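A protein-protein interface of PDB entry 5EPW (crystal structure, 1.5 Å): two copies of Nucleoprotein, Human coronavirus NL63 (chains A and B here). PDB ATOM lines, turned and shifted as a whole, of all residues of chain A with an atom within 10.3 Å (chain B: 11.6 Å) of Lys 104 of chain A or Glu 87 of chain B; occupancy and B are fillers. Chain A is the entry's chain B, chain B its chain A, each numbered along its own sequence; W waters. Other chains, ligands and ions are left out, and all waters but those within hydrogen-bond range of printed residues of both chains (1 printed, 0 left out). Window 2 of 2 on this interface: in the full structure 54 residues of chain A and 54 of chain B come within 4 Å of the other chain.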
ATOM      1  N   LEU A  70      28.144  -4.024   1.827  1.00  0.00           N
ATOM      2  CA  LEU A  70      27.373  -4.390   0.618  1.00  0.00           C
ATOM      3  C   LEU A  70      28.262  -5.073  -0.470  1.00  0.00           C
ATOM      4  O   LEU A  70      27.878  -5.152  -1.615  1.00  0.00           O
ATOM      5  CB  LEU A  70      26.601  -3.267   0.025  1.00  0.00           C
ATOM      6  CG  LEU A  70      25.478  -2.725   0.916  1.00  0.00           C
ATOM      7  CD1 LEU A  70      24.762  -1.654   0.222  1.00  0.00           C
ATOM      8  CD2 LEU A  70      24.541  -3.814   1.493  1.00  0.00           C
ATOM      9  N   MET A 100      22.649  -9.460  -6.094  1.00  0.00           N
ATOM     10  CA  MET A 100      22.160  -9.433  -4.682  1.00  0.00           C
ATOM     11  C   MET A 100      21.037  -8.446  -4.581  1.00  0.00           C
ATOM     12  O   MET A 100      21.010  -7.371  -5.212  1.00  0.00           O
ATOM     13  CB  MET A 100      23.272  -9.091  -3.702  1.00  0.00           C
ATOM     14  CG  MET A 100      24.035  -7.804  -4.028  1.00  0.00           C
ATOM     15  SD  MET A 100      25.504  -7.493  -3.012  1.00  0.00           S
ATOM     16  CE  MET A 100      24.778  -6.529  -1.642  1.00  0.00           C
ATOM     17  N   LEU A 101      20.022  -8.906  -3.810  1.00  0.00           N
ATOM     18  CA  LEU A 101      18.821  -8.033  -3.513  1.00  0.00           C
ATOM     19  C   LEU A 101      18.980  -7.309  -2.138  1.00  0.00           C
ATOM     20  O   LEU A 101      19.099  -7.998  -1.114  1.00  0.00           O
ATOM     21  CB  LEU A 101      17.537  -8.936  -3.480  1.00  0.00           C
ATOM     22  CG  LEU A 101      17.190  -9.524  -4.820  1.00  0.00           C
ATOM     23  CD1 LEU A 101      16.066 -10.570  -4.636  1.00  0.00           C
ATOM     24  CD2 LEU A 101      16.846  -8.491  -5.834  1.00  0.00           C
ATOM     25  N   VAL A 102      19.032  -5.993  -2.202  1.00  0.00           N
ATOM     26  CA  VAL A 102      19.176  -5.212  -0.988  1.00  0.00           C
ATOM     27  C   VAL A 102      17.823  -4.468  -0.715  1.00  0.00           C
ATOM     28  O   VAL A 102      17.314  -3.821  -1.564  1.00  0.00           O
ATOM     29  CB  VAL A 102      20.267  -4.227  -1.155  1.00  0.00           C
ATOM     30  CG1 VAL A 102      20.546  -3.518   0.102  1.00  0.00           C
ATOM     31  CG2 VAL A 102      21.572  -4.945  -1.531  1.00  0.00           C
ATOM     32  N   ALA A 103      17.320  -4.624   0.542  1.00  0.00           N
ATOM     33  CA  ALA A 103      16.095  -3.931   0.938  1.00  0.00           C
ATOM     34  C   ALA A 103      16.230  -2.448   0.765  1.00  0.00           C
ATOM     35  O   ALA A 103      17.301  -1.863   1.046  1.00  0.00           O
ATOM     36  CB  ALA A 103      15.753  -4.333   2.389  1.00  0.00           C
ATOM     37  N   LYS A 104      15.191  -1.776   0.247  1.00  0.00           N
ATOM     38  CA  LYS A 104      15.256  -0.348   0.011  1.00  0.00           C
ATOM     39  C   LYS A 104      15.467   0.533   1.268  1.00  0.00           C
ATOM     40  O   LYS A 104      15.982   1.662   1.144  1.00  0.00           O
ATOM     41  CB  LYS A 104      13.962   0.146  -0.743  1.00  0.00           C
ATOM     42  CG  LYS A 104      14.106  -0.147  -2.234  1.00  0.00           C
ATOM     43  CD  LYS A 104      12.777   0.062  -2.924  1.00  0.00           C
ATOM     44  CE  LYS A 104      12.920  -0.139  -4.421  1.00  0.00           C
ATOM     45  NZ  LYS A 104      11.584  -0.026  -5.029  1.00  0.00           N
ATOM     46  N   ASP A 105      15.207  -0.047   2.407  1.00  0.00           N
ATOM     47  CA  ASP A 105      15.432   0.644   3.643  1.00  0.00           C
ATOM     48  C   ASP A 105      16.759   0.302   4.302  1.00  0.00           C
ATOM     49  O   ASP A 105      17.026   0.703   5.454  1.00  0.00           O
ATOM     50  CB  ASP A 105      14.210   0.479   4.542  1.00  0.00           C
ATOM     51  CG  ASP A 105      14.085  -0.875   5.145  1.00  0.00           C
ATOM     52  OD1 ASP A 105      14.483  -1.907   4.589  1.00  0.00           O
ATOM     53  OD2 ASP A 105      13.537  -0.949   6.260  1.00  0.00           O
ATOM     54  N   ASN A 106      17.624  -0.464   3.580  1.00  0.00           N
ATOM     55  CA  ASN A 106      18.915  -0.742   4.088  1.00  0.00           C
ATOM     56  C   ASN A 106      19.639   0.580   4.206  1.00  0.00           C
ATOM     57  O   ASN A 106      19.751   1.341   3.294  1.00  0.00           O
ATOM     58  CB  ASN A 106      19.663  -1.688   3.123  1.00  0.00           C
ATOM     59  CG  ASN A 106      21.021  -2.065   3.671  1.00  0.00           C
ATOM     60  OD1 ASN A 106      21.856  -1.168   3.816  1.00  0.00           O
ATOM     61  ND2 ASN A 106      21.285  -3.338   3.823  1.00  0.00           N
ATOM     62  N   LYS A 107      20.208   0.804   5.426  1.00  0.00           N
ATOM     63  CA  LYS A 107      20.797   2.085   5.684  1.00  0.00           C
ATOM     64  C   LYS A 107      22.137   2.333   5.008  1.00  0.00           C
ATOM     65  O   LYS A 107      22.604   3.401   4.933  1.00  0.00           O
ATOM     66  CB  LYS A 107      20.995   2.256   7.221  1.00  0.00           C
ATOM     67  CG  LYS A 107      19.713   2.535   8.014  1.00  0.00           C
ATOM     68  CD  LYS A 107      20.035   2.636   9.544  1.00  0.00           C
ATOM     69  CE  LYS A 107      18.979   2.009  10.429  1.00  0.00           C
ATOM     70  NZ  LYS A 107      17.623   2.133   9.884  1.00  0.00           N
ATOM     71  N   ASN A 108      22.712   1.268   4.481  1.00  0.00           N
ATOM     72  CA  ASN A 108      23.999   1.357   3.797  1.00  0.00           C
ATOM     73  C   ASN A 108      23.851   1.505   2.305  1.00  0.00           C
ATOM     74  O   ASN A 108      24.806   1.852   1.627  1.00  0.00           O
ATOM     75  CB  ASN A 108      24.779   0.108   4.142  1.00  0.00           C
ATOM     76  CG  ASN A 108      25.026  -0.036   5.623  1.00  0.00           C
ATOM     77  OD1 ASN A 108      25.362   0.954   6.326  1.00  0.00           O
ATOM     78  ND2 ASN A 108      24.896  -1.227   6.139  1.00  0.00           N
ATOM     79  N   LEU A 109      22.659   1.337   1.800  1.00  0.00           N
ATOM     80  CA  LEU A 109      22.412   1.370   0.365  1.00  0.00           C
ATOM     81  C   LEU A 109      22.659   2.767  -0.258  1.00  0.00           C
ATOM     82  O   LEU A 109      23.256   2.989  -1.321  1.00  0.00           O
ATOM     83  CB  LEU A 109      20.996   0.817   0.032  1.00  0.00           C
ATOM     84  CG  LEU A 109      20.545   0.741  -1.388  1.00  0.00           C
ATOM     85  CD1 LEU A 109      21.450  -0.174  -2.246  1.00  0.00           C
ATOM     86  CD2 LEU A 109      19.129   0.229  -1.379  1.00  0.00           C
ATOM     87  N   PRO A 110      22.207   3.885   0.398  1.00  0.00           N
ATOM     88  CA  PRO A 110      22.432   5.143  -0.252  1.00  0.00           C
ATOM     89  C   PRO A 110      23.918   5.518  -0.489  1.00  0.00           C
ATOM     90  O   PRO A 110      24.231   6.097  -1.512  1.00  0.00           O
ATOM     91  CB  PRO A 110      21.802   6.177   0.717  1.00  0.00           C
ATOM     92  CG  PRO A 110      20.822   5.359   1.434  1.00  0.00           C
ATOM     93  CD  PRO A 110      21.317   3.970   1.597  1.00  0.00           C
ATOM     94  N   LYS A 111      24.784   5.179   0.475  1.00  0.00           N
ATOM     95  CA  LYS A 111      26.231   5.398   0.292  1.00  0.00           C
ATOM     96  C   LYS A 111      26.775   4.602  -0.920  1.00  0.00           C
ATOM     97  O   LYS A 111      27.574   5.125  -1.674  1.00  0.00           O
ATOM     98  CB  LYS A 111      26.906   4.913   1.548  1.00  0.00           C
ATOM     99  CG  LYS A 111      28.471   5.008   1.559  1.00  0.00           C
ATOM    100  CD  LYS A 111      28.938   6.417   1.390  1.00  0.00           C
ATOM    101  CE  LYS A 111      30.451   6.600   1.589  1.00  0.00           C
ATOM    102  NZ  LYS A 111      30.780   8.056   1.450  1.00  0.00           N
ATOM    103  N   ILE A 113      25.055   3.592  -3.600  1.00  0.00           N
ATOM    104  CA  ILE A 113      24.585   4.186  -4.787  1.00  0.00           C
ATOM    105  C   ILE A 113      25.307   5.451  -5.193  1.00  0.00           C
ATOM    106  O   ILE A 113      25.599   5.698  -6.367  1.00  0.00           O
ATOM    107  CB  ILE A 113      23.008   4.370  -4.667  1.00  0.00           C
ATOM    108  CG1 ILE A 113      22.309   3.032  -4.721  1.00  0.00           C
ATOM    109  CG2 ILE A 113      22.563   5.196  -5.867  1.00  0.00           C
ATOM    110  CD1 ILE A 113      20.822   3.020  -4.380  1.00  0.00           C
ATOM    111  N   TRP B  26      24.645 -12.195   0.937  1.00  0.00           N
ATOM    112  CA  TRP B  26      25.989 -11.879   0.462  1.00  0.00           C
ATOM    113  C   TRP B  26      27.044 -12.030   1.539  1.00  0.00           C
ATOM    114  O   TRP B  26      28.268 -11.927   1.202  1.00  0.00           O
ATOM    115  CB  TRP B  26      26.048 -10.504  -0.191  1.00  0.00           C
ATOM    116  CG  TRP B  26      25.619  -9.347   0.723  1.00  0.00           C
ATOM    117  CD1 TRP B  26      26.404  -8.496   1.352  1.00  0.00           C
ATOM    118  CD2 TRP B  26      24.285  -8.814   0.894  1.00  0.00           C
ATOM    119  NE1 TRP B  26      25.682  -7.570   2.066  1.00  0.00           N
ATOM    120  CE2 TRP B  26      24.368  -7.717   1.755  1.00  0.00           C
ATOM    121  CE3 TRP B  26      23.036  -9.192   0.374  1.00  0.00           C
ATOM    122  CZ2 TRP B  26      23.268  -6.976   2.128  1.00  0.00           C
ATOM    123  CZ3 TRP B  26      21.926  -8.452   0.753  1.00  0.00           C
ATOM    124  CH2 TRP B  26      22.066  -7.380   1.634  1.00  0.00           C
ATOM    125  N   SER B  84      26.039  -2.495 -11.687  1.00  0.00           N
ATOM    126  CA  SER B  84      24.744  -1.934 -12.211  1.00  0.00           C
ATOM    127  C   SER B  84      23.658  -2.239 -11.240  1.00  0.00           C
ATOM    128  O   SER B  84      23.779  -3.102 -10.352  1.00  0.00           O
ATOM    129  CB  SER B  84      24.447  -2.547 -13.568  1.00  0.00           C
ATOM    130  OG  SER B  84      24.387  -3.956 -13.527  1.00  0.00           O
ATOM    131  N   THR B  85      22.475  -1.526 -11.399  1.00  0.00           N
ATOM    132  CA  THR B  85      21.397  -1.679 -10.428  1.00  0.00           C
ATOM    133  C   THR B  85      20.056  -1.712 -11.155  1.00  0.00           C
ATOM    134  O   THR B  85      19.940  -1.183 -12.249  1.00  0.00           O
ATOM    135  CB  THR B  85      21.268  -0.584  -9.326  1.00  0.00           C
ATOM    136  OG1 THR B  85      20.981   0.658  -9.977  1.00  0.00           O
ATOM    137  CG2 THR B  85      22.487  -0.488  -8.407  1.00  0.00           C
ATOM    138  N   ASP B  86      19.097  -2.401 -10.522  1.00  0.00           N
ATOM    139  CA  ASP B  86      17.711  -2.415 -11.035  1.00  0.00           C
ATOM    140  C   ASP B  86      16.811  -2.468  -9.831  1.00  0.00           C
ATOM    141  O   ASP B  86      17.114  -3.091  -8.870  1.00  0.00           O
ATOM    142  CB  ASP B  86      17.539  -3.750 -11.747  1.00  0.00           C
ATOM    143  CG  ASP B  86      17.026  -3.650 -13.035  1.00  0.00           C
ATOM    144  OD1 ASP B  86      17.808  -3.092 -13.896  1.00  0.00           O
ATOM    145  OD2 ASP B  86      15.911  -4.305 -13.169  1.00  0.00           O
ATOM    146  N   GLU B  87      15.600  -1.844  -9.922  1.00  0.00           N
ATOM    147  CA  GLU B  87      14.555  -1.988  -8.877  1.00  0.00           C
ATOM    148  C   GLU B  87      13.712  -3.233  -9.022  1.00  0.00           C
ATOM    149  O   GLU B  87      13.319  -3.560 -10.117  1.00  0.00           O
ATOM    150  CB  GLU B  87      13.677  -0.741  -9.005  1.00  0.00           C
ATOM    151  CG  GLU B  87      14.410   0.496  -8.450  1.00  0.00           C
ATOM    152  CD  GLU B  87      13.418   1.611  -8.099  1.00  0.00           C
ATOM    153  OE1 GLU B  87      12.451   1.346  -7.308  1.00  0.00           O
ATOM    154  OE2 GLU B  87      13.578   2.723  -8.663  1.00  0.00           O
ATOM    155  N   VAL B  88      13.562  -4.045  -7.982  1.00  0.00           N
ATOM    156  CA  VAL B  88      12.832  -5.249  -8.010  1.00  0.00           C
ATOM    157  C   VAL B  88      11.965  -5.240  -6.723  1.00  0.00           C
ATOM    158  O   VAL B  88      12.475  -5.559  -5.617  1.00  0.00           O
ATOM    159  CB  VAL B  88      13.748  -6.482  -8.007  1.00  0.00           C
ATOM    160  CG1 VAL B  88      12.949  -7.790  -8.030  1.00  0.00           C
ATOM    161  CG2 VAL B  88      14.727  -6.447  -9.192  1.00  0.00           C
ATOM    162  N   GLY B  89      10.638  -4.933  -6.871  1.00  0.00           N
ATOM    163  CA  GLY B  89       9.815  -4.795  -5.631  1.00  0.00           C
ATOM    164  C   GLY B  89      10.429  -3.842  -4.589  1.00  0.00           C
ATOM    165  O   GLY B  89      10.684  -2.680  -4.868  1.00  0.00           O
ATOM    166  N   ASP B  90      10.581  -4.363  -3.373  1.00  0.00           N
ATOM    167  CA  ASP B  90      11.063  -3.499  -2.256  1.00  0.00           C
ATOM    168  C   ASP B  90      12.579  -3.630  -2.111  1.00  0.00           C
ATOM    169  O   ASP B  90      13.109  -3.454  -1.023  1.00  0.00           O
ATOM    170  CB  ASP B  90      10.433  -3.965  -0.934  1.00  0.00           C
ATOM    171  CG  ASP B  90      10.760  -3.069   0.226  1.00  0.00           C
ATOM    172  OD1 ASP B  90      10.682  -1.819   0.058  1.00  0.00           O
ATOM    173  OD2 ASP B  90      11.064  -3.699   1.296  1.00  0.00           O
ATOM    174  N   ASN B  91      13.220  -4.052  -3.189  1.00  0.00           N
ATOM    175  CA  ASN B  91      14.714  -4.214  -3.184  1.00  0.00           C
ATOM    176  C   ASN B  91      15.317  -3.454  -4.298  1.00  0.00           C
ATOM    177  O   ASN B  91      14.705  -3.139  -5.317  1.00  0.00           O
ATOM    178  CB  ASN B  91      15.023  -5.688  -3.411  1.00  0.00           C
ATOM    179  CG  ASN B  91      14.431  -6.573  -2.380  1.00  0.00           C
ATOM    180  OD1 ASN B  91      13.535  -7.434  -2.656  1.00  0.00           O
ATOM    181  ND2 ASN B  91      14.887  -6.411  -1.192  1.00  0.00           N
ATOM    182  N   VAL B  92      16.622  -3.148  -4.135  1.00  0.00           N
ATOM    183  CA  VAL B  92      17.478  -2.796  -5.262  1.00  0.00           C
ATOM    184  C   VAL B  92      18.431  -4.045  -5.508  1.00  0.00           C
ATOM    185  O   VAL B  92      19.028  -4.600  -4.575  1.00  0.00           O
ATOM    186  CB  VAL B  92      18.337  -1.598  -4.940  1.00  0.00           C
ATOM    187  CG1 VAL B  92      19.346  -1.276  -6.027  1.00  0.00           C
ATOM    188  CG2 VAL B  92      17.451  -0.354  -4.689  1.00  0.00           C
ATOM    189  N   GLN B  93      18.369  -4.497  -6.752  1.00  0.00           N
ATOM    190  CA  GLN B  93      19.236  -5.606  -7.248  1.00  0.00           C
ATOM    191  C   GLN B  93      20.561  -4.900  -7.706  1.00  0.00           C
ATOM    192  O   GLN B  93      20.561  -4.132  -8.663  1.00  0.00           O
ATOM    193  CB  GLN B  93      18.614  -6.339  -8.394  1.00  0.00           C
ATOM    194  CG  GLN B  93      19.473  -7.547  -8.809  1.00  0.00           C
ATOM    195  CD  GLN B  93      19.039  -8.090 -10.196  1.00  0.00           C
ATOM    196  OE1 GLN B  93      18.996  -7.353 -11.174  1.00  0.00           O
ATOM    197  NE2 GLN B  93      18.615  -9.231 -10.201  1.00  0.00           N
ATOM    198  N   ILE B  94      21.655  -5.296  -7.027  1.00  0.00           N
ATOM    199  CA  ILE B  94      23.000  -4.873  -7.393  1.00  0.00           C
ATOM    200  C   ILE B  94      23.628  -6.109  -8.132  1.00  0.00           C
ATOM    201  O   ILE B  94      23.636  -7.218  -7.625  1.00  0.00           O
ATOM    202  CB  ILE B  94      23.864  -4.551  -6.174  1.00  0.00           C
ATOM    203  CG1 ILE B  94      23.203  -3.412  -5.326  1.00  0.00           C
ATOM    204  CG2 ILE B  94      25.282  -4.128  -6.647  1.00  0.00           C
ATOM    205  CD1 ILE B  94      23.928  -3.094  -4.032  1.00  0.00           C
ATOM    206  N   THR B  95      24.111  -5.808  -9.367  1.00  0.00           N
ATOM    207  CA  THR B  95      24.839  -6.775 -10.211  1.00  0.00           C
ATOM    208  C   THR B  95      26.269  -6.351 -10.265  1.00  0.00           C
ATOM    209  O   THR B  95      26.632  -5.289 -10.772  1.00  0.00           O
ATOM    210  CB  THR B  95      24.253  -6.941 -11.611  1.00  0.00           C
ATOM    211  OG1 THR B  95      22.859  -7.297 -11.499  1.00  0.00           O
ATOM    212  CG2 THR B  95      25.015  -8.110 -12.337  1.00  0.00           C
HETATM  213  O   HOH W   1      16.370  -8.415   0.326  1.00  0.00           O
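Of the 14 printed residues of chain A, 7 touch a printed residue of chain B.
Hydrophobic or aromatic side chains of chain A that line the printed part of chain B: Leu 70, Met 100, Leu 101, Val 102 and Leu 109.
Printed residues of chain B that touch a printed residue of chain A: Trp 26, Glu 87, Gly 89, Asp 90, Asn 91, Val 92, Gln 93 and Ile 94.
Among the printed residues, Asp or Glu carboxylates within 4 Å of a Lys or Arg side-chain nitrogen of the other chain: Lys 104 of chain A with Glu 87 of chain B.
Of chain B, only Glu 87 (2.8 Å), Gly 89 (2.8 Å), Asp 90 (3.0 Å) and Asn 91 (3.6 Å) come within 4 Å of Lys 104 of chain A.
Glu 87 of chain B touches just one residue of chain A: Lys 104.
Val 102 of chain A touches three residues of chain B.
Ala 103 of chain A touches two residues of chain B.
No residue of chain B comes within 4 Å of Asp 105 of chain A.
No residue of chain B comes within 4 Å of Asn 106 of chain A.
No residue of chain A comes within 4 Å of Asp 86 of chain B.
No residue of chain A comes within 4 Å of Val 88 of chain B.
Gly 89 of chain B touches one residue of chain A.
Of chain A, only Ala 103 and Lys 104 come within 4 Å of Asp 90 of chain B.
Of the printed residues of chain A, Trp 26 of chain B touches Leu 70, Met 100 and Leu 101.
Of the printed residues of chain B, Leu 70 of chain A touches Trp 26 (3.5 Å).
Printed residues of chain A within 4 Å of Gln 93 of chain B: Met 100 and Leu 101.
Of the printed residues of chain A, Ile 94 of chain B touches Met 100 and Val 102.
Lys 111 of chain A touches none of the printed residues of chain B.
Thr 95 of chain B touches none of the printed residues of chain A.
The nearest residue of chain A that does not touch Glu 87 of chain B is Leu 101 of chain A (6.9 Å).
The nearest printed residue of chain B that does not touch Leu 70 of chain A is Ile 94 of chain B (4.6 Å).
The side-chain carboxylate (OE1) of Glu 87 of chain B is in salt-bridge range of the side-chain amino group (NZ) of Lys 104 of chain A, at 2.8 Å.
The side-chain amino group (NZ) of Lys 104 of chain A is in hydrogen-bond range of the backbone carbonyl oxygen (O) of Gly 89 of chain B.
O of Asp 90 of chain B lies within hydrogen-bond range of N of Lys 104 of chain A (3.0 Å).
ND2 of Asn 91 of chain B sits close to N of Ala 103 of chain A, 3.5 Å away.
The backbone carbonyl oxygen (O) of Val 102 of chain A is in hydrogen-bond range of the backbone NH (N) of Val 92 of chain B (2.7 Å).
The backbone carbonyl oxygen (O) of Met 100 of chain A sits at hydrogen-bond distance from the backbone NH (N) of Ile 94 of chain B.
The backbone carbonyl oxygen (O) of Val 92 of chain B lies close to the backbone carbonyl oxygen (O) of Met 100 of chain A (3.5 Å).
Water W1 lies within hydrogen-bond range of the side-chain amide nitrogen of Asn 91 of chain B (2.9 Å) and the backbone carbonyl oxygen of Leu 101 of chain A (3.1 Å).
No position is printed for both chains.
The backbone carbonyl oxygen of Asp 86 of chain B sits at hydrogen-bond distance from the backbone NH of Gln 93 of chain B (2.8 Å).
N of Leu 109 of chain A is in hydrogen-bond range of OD1 of Asn 106 of chain A (3.3 Å).
Among the printed residues, pairs that only touch across the chains: Leu 70 of chain A with Trp 26 of chain B, Met 100 of chain A with Trp 26 of chain B, Met 100 of chain A with Gln 93 of chain B, Leu 101 of chain A with Trp 26 of chain B, Leu 101 of chain A with Val 92 of chain B, Leu 101 of chain A with Gln 93 of chain B, Val 102 of chain A with Asn 91 of chain B, Val 102 of chain A with Ile 94 of chain B, Ala 103 of chain A with Asp 90 of chain B, Lys 104 of chain A with Asn 91 of chain B and Leu 109 of chain A with Val 92 of chain B.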
